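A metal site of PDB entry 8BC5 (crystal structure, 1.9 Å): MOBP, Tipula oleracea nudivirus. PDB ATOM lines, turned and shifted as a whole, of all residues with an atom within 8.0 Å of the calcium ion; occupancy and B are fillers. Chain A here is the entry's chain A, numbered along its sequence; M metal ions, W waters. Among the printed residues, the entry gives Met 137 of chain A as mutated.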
ATOM      1  N   SER A 136     -19.912  -0.994  -6.150  1.00  0.00           N
ATOM      2  CA  SER A 136     -20.071   0.437  -5.915  1.00  0.00           C
ATOM      3  C   SER A 136     -19.263   1.253  -6.916  1.00  0.00           C
ATOM      4  O   SER A 136     -19.716   2.310  -7.375  1.00  0.00           O
ATOM      5  CB  SER A 136     -19.663   0.763  -4.475  1.00  0.00           C
ATOM      6  OG  SER A 136     -19.677   2.157  -4.242  1.00  0.00           O
ATOM      7  N   MET A 137     -18.063   0.790  -7.274  1.00  0.00           N
ATOM      8  CA  MET A 137     -17.228   1.506  -8.239  1.00  0.00           C
ATOM      9  C   MET A 137     -17.883   1.494  -9.622  1.00  0.00           C
ATOM     10  O   MET A 137     -17.891   2.520 -10.302  1.00  0.00           O
ATOM     11  CB  MET A 137     -15.837   0.913  -8.229  1.00  0.00           C
ATOM     12  CG  MET A 137     -14.801   1.378  -9.258  1.00  0.00           C
ATOM     13  SD  MET A 137     -15.083   0.843 -11.060  1.00  0.00           S
ATOM     14  CE  MET A 137     -14.369  -0.964 -11.004  1.00  0.00           C
ATOM     15  N   ILE A 138     -18.462   0.357 -10.023  1.00  0.00           N
ATOM     16  CA  ILE A 138     -19.093   0.288 -11.331  1.00  0.00           C
ATOM     17  C   ILE A 138     -20.345   1.174 -11.385  1.00  0.00           C
ATOM     18  O   ILE A 138     -20.604   1.834 -12.391  1.00  0.00           O
ATOM     19  CB  ILE A 138     -19.428  -1.163 -11.711  1.00  0.00           C
ATOM     20  CG1 ILE A 138     -18.181  -2.020 -11.836  1.00  0.00           C
ATOM     21  CG2 ILE A 138     -20.207  -1.192 -13.002  1.00  0.00           C
ATOM     22  CD1 ILE A 138     -18.468  -3.494 -11.640  1.00  0.00           C
ATOM     23  N   CYS A 139     -21.147   1.186 -10.315  1.00  0.00           N
ATOM     24  CA  CYS A 139     -22.302   2.084 -10.268  1.00  0.00           C
ATOM     25  C   CYS A 139     -21.871   3.539 -10.452  1.00  0.00           C
ATOM     26  O   CYS A 139     -22.545   4.314 -11.137  1.00  0.00           O
ATOM     27  CB  CYS A 139     -23.034   1.912  -8.926  1.00  0.00           C
ATOM     28  SG  CYS A 139     -23.940   0.357  -8.744  1.00  0.00           S
ATOM     29  N   ASP A 140     -20.751   3.910  -9.833  1.00  0.00           N
ATOM     30  CA  ASP A 140     -20.217   5.258  -9.974  1.00  0.00           C
ATOM     31  C   ASP A 140     -19.738   5.502 -11.398  1.00  0.00           C
ATOM     32  O   ASP A 140     -20.080   6.530 -12.001  1.00  0.00           O
ATOM     33  CB  ASP A 140     -19.107   5.448  -8.923  1.00  0.00           C
ATOM     34  CG  ASP A 140     -18.505   6.840  -8.909  1.00  0.00           C
ATOM     35  OD1 ASP A 140     -18.987   7.724  -9.659  1.00  0.00           O
ATOM     36  OD2 ASP A 140     -17.552   7.058  -8.124  1.00  0.00           O
ATOM     37  N   PHE A 141     -19.022   4.548 -11.985  1.00  0.00           N
ATOM     38  CA  PHE A 141     -18.609   4.707 -13.365  1.00  0.00           C
ATOM     39  C   PHE A 141     -19.798   5.029 -14.268  1.00  0.00           C
ATOM     40  O   PHE A 141     -19.734   5.954 -15.095  1.00  0.00           O
ATOM     41  CB  PHE A 141     -17.889   3.437 -13.836  1.00  0.00           C
ATOM     42  CG  PHE A 141     -17.108   3.609 -15.112  1.00  0.00           C
ATOM     43  CD1 PHE A 141     -17.724   3.540 -16.347  1.00  0.00           C
ATOM     44  CD2 PHE A 141     -15.734   3.845 -15.066  1.00  0.00           C
ATOM     45  CE1 PHE A 141     -16.987   3.683 -17.511  1.00  0.00           C
ATOM     46  CE2 PHE A 141     -15.002   3.996 -16.226  1.00  0.00           C
ATOM     47  CZ  PHE A 141     -15.629   3.915 -17.448  1.00  0.00           C
ATOM     48  N   LYS A 142     -20.916   4.326 -14.083  1.00  0.00           N
ATOM     49  CA  LYS A 142     -22.015   4.350 -15.038  1.00  0.00           C
ATOM     50  C   LYS A 142     -23.117   5.352 -14.683  1.00  0.00           C
ATOM     51  O   LYS A 142     -24.086   5.465 -15.440  1.00  0.00           O
ATOM     52  CB  LYS A 142     -22.615   2.944 -15.156  1.00  0.00           C
ATOM     53  CG  LYS A 142     -21.605   1.907 -15.613  1.00  0.00           C
ATOM     54  CD  LYS A 142     -22.164   0.495 -15.581  1.00  0.00           C
ATOM     55  CE  LYS A 142     -21.224  -0.483 -16.286  1.00  0.00           C
ATOM     56  NZ  LYS A 142     -21.799  -1.861 -16.376  1.00  0.00           N
ATOM     57  N   ASN A 143     -22.993   6.089 -13.580  1.00  0.00           N
ATOM     58  CA  ASN A 143     -24.093   6.976 -13.190  1.00  0.00           C
ATOM     59  C   ASN A 143     -24.196   8.236 -14.037  1.00  0.00           C
ATOM     60  O   ASN A 143     -25.210   8.938 -13.925  1.00  0.00           O
ATOM     61  CB  ASN A 143     -24.053   7.296 -11.678  1.00  0.00           C
ATOM     62  CG  ASN A 143     -22.806   8.070 -11.246  1.00  0.00           C
ATOM     63  OD1 ASN A 143     -22.175   8.773 -12.018  1.00  0.00           O
ATOM     64  ND2 ASN A 143     -22.529   8.002  -9.943  1.00  0.00           N
ATOM     65  N   THR A 144     -23.238   8.521 -14.917  1.00  0.00           N
ATOM     66  CA  THR A 144     -23.348   9.580 -15.909  1.00  0.00           C
ATOM     67  C   THR A 144     -22.598   9.138 -17.151  1.00  0.00           C
ATOM     68  O   THR A 144     -21.581   8.450 -17.046  1.00  0.00           O
ATOM     69  CB  THR A 144     -22.759  10.916 -15.410  1.00  0.00           C
ATOM     70  OG1 THR A 144     -21.368  10.724 -15.122  1.00  0.00           O
ATOM     71  CG2 THR A 144     -23.485  11.386 -14.170  1.00  0.00           C
ATOM     72  N   PRO A 145     -23.070   9.516 -18.347  1.00  0.00           N
ATOM     73  CA  PRO A 145     -22.298   9.174 -19.558  1.00  0.00           C
ATOM     74  C   PRO A 145     -20.904   9.764 -19.544  1.00  0.00           C
ATOM     75  O   PRO A 145     -19.959   9.111 -19.991  1.00  0.00           O
ATOM     76  CB  PRO A 145     -23.170   9.722 -20.697  1.00  0.00           C
ATOM     77  CG  PRO A 145     -24.539   9.768 -20.120  1.00  0.00           C
ATOM     78  CD  PRO A 145     -24.359  10.159 -18.685  1.00  0.00           C
ATOM     79  N   TRP A 146     -20.752  10.991 -19.057  1.00  0.00           N
ATOM     80  CA  TRP A 146     -19.422  11.540 -18.817  1.00  0.00           C
ATOM     81  C   TRP A 146     -18.809  10.830 -17.619  1.00  0.00           C
ATOM     82  O   TRP A 146     -19.408  10.763 -16.545  1.00  0.00           O
ATOM     83  CB  TRP A 146     -19.528  13.046 -18.566  1.00  0.00           C
ATOM     84  CG  TRP A 146     -18.217  13.681 -18.323  1.00  0.00           C
ATOM     85  CD1 TRP A 146     -17.569  13.783 -17.143  1.00  0.00           C
ATOM     86  CD2 TRP A 146     -17.383  14.315 -19.302  1.00  0.00           C
ATOM     87  NE1 TRP A 146     -16.374  14.438 -17.313  1.00  0.00           N
ATOM     88  CE2 TRP A 146     -16.235  14.777 -18.626  1.00  0.00           C
ATOM     89  CE3 TRP A 146     -17.491  14.533 -20.680  1.00  0.00           C
ATOM     90  CZ2 TRP A 146     -15.202  15.436 -19.290  1.00  0.00           C
ATOM     91  CZ3 TRP A 146     -16.465  15.189 -21.321  1.00  0.00           C
ATOM     92  CH2 TRP A 146     -15.333  15.634 -20.626  1.00  0.00           C
ATOM     93  N   ILE A 147     -17.610  10.278 -17.811  1.00  0.00           N
ATOM     94  CA  ILE A 147     -16.980   9.464 -16.774  1.00  0.00           C
ATOM     95  C   ILE A 147     -16.357  10.358 -15.707  1.00  0.00           C
ATOM     96  O   ILE A 147     -15.467  11.158 -15.991  1.00  0.00           O
ATOM     97  CB  ILE A 147     -15.944   8.498 -17.348  1.00  0.00           C
ATOM     98  CG1 ILE A 147     -16.611   7.536 -18.325  1.00  0.00           C
ATOM     99  CG2 ILE A 147     -15.270   7.719 -16.246  1.00  0.00           C
ATOM    100  CD1 ILE A 147     -15.677   6.970 -19.355  1.00  0.00           C
ATOM    101  N   ASN A 148     -16.798  10.185 -14.471  1.00  0.00           N
ATOM    102  CA  ASN A 148     -16.248  10.880 -13.315  1.00  0.00           C
ATOM    103  C   ASN A 148     -16.337   9.913 -12.156  1.00  0.00           C
ATOM    104  O   ASN A 148     -17.434   9.447 -11.831  1.00  0.00           O
ATOM    105  CB  ASN A 148     -17.036  12.162 -13.041  1.00  0.00           C
ATOM    106  CG  ASN A 148     -16.388  13.042 -11.968  1.00  0.00           C
ATOM    107  OD1 ASN A 148     -15.692  12.553 -11.080  1.00  0.00           O
ATOM    108  ND2 ASN A 148     -16.586  14.346 -12.082  1.00  0.00           N
ATOM    109  N   LEU A 149     -15.198   9.551 -11.563  1.00  0.00           N
ATOM    110  CA  LEU A 149     -15.176   8.646 -10.417  1.00  0.00           C
ATOM    111  C   LEU A 149     -14.756   9.390  -9.160  1.00  0.00           C
ATOM    112  O   LEU A 149     -13.920  10.296  -9.200  1.00  0.00           O
ATOM    113  CB  LEU A 149     -14.210   7.480 -10.653  1.00  0.00           C
ATOM    114  CG  LEU A 149     -14.643   6.415 -11.670  1.00  0.00           C
ATOM    115  CD1 LEU A 149     -13.570   5.340 -11.771  1.00  0.00           C
ATOM    116  CD2 LEU A 149     -15.967   5.773 -11.290  1.00  0.00           C
ATOM    117  N   SER A 150     -15.327   8.996  -8.023  1.00  0.00           N
ATOM    118  CA  SER A 150     -14.842   9.520  -6.749  1.00  0.00           C
ATOM    119  C   SER A 150     -13.393   9.069  -6.532  1.00  0.00           C
ATOM    120  O   SER A 150     -12.917   8.119  -7.143  1.00  0.00           O
ATOM    121  CB  SER A 150     -15.704   9.021  -5.604  1.00  0.00           C
ATOM    122  OG  SER A 150     -15.460   7.648  -5.363  1.00  0.00           O
ATOM    123  N   HIS A 153     -13.058   5.499  -5.665  1.00  0.00           N
ATOM    124  CA  HIS A 153     -13.413   4.611  -6.771  1.00  0.00           C
ATOM    125  C   HIS A 153     -12.361   4.610  -7.861  1.00  0.00           C
ATOM    126  O   HIS A 153     -12.241   3.614  -8.597  1.00  0.00           O
ATOM    127  CB  HIS A 153     -14.769   5.019  -7.316  1.00  0.00           C
ATOM    128  CG  HIS A 153     -15.931   4.593  -6.456  1.00  0.00           C
ATOM    129  ND1 HIS A 153     -17.125   5.270  -6.442  1.00  0.00           N
ATOM    130  CD2 HIS A 153     -16.061   3.570  -5.583  1.00  0.00           C
ATOM    131  CE1 HIS A 153     -17.957   4.666  -5.605  1.00  0.00           C
ATOM    132  NE2 HIS A 153     -17.335   3.638  -5.068  1.00  0.00           N
HETATM  133 CA    CA M   1     -19.720   8.950 -11.673  1.00  0.00          CA
HETATM  134  O   HOH W   1     -19.349   8.570 -14.254  1.00  0.00           O
HETATM  135  O   HOH W   2     -20.497  11.151 -12.583  1.00  0.00           O
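OD2 of Asp 140 is in hydrogen-bond range of N of Ser 150, at 3.0 Å. A ring nitrogen (ND1) of His 153 lies within hydrogen-bond range of the side-chain carboxylate (OD2) of Asp 140 (2.5 Å).
The nearest printed residue that does not touch the calcium ion is Thr 144 (4.2 Å).
O of Asn 148 is bound to the calcium ion (2.3 Å). OD1 of Asp 140 binds the calcium ion (2.5 Å). O of Asp 140 is bound to the calcium ion, at 2.5 Å. The side-chain amide oxygen (OD1) of Asn 143 is bound to the calcium ion, at 2.5 Å. Water W2 is bound to the calcium ion (2.5 Å). Water W1 binds the calcium ion (2.6 Å).
Water W1 lies within hydrogen-bond range of O of Phe 141, N of Asn 148, OG1 of Thr 144 and O of Trp 146.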
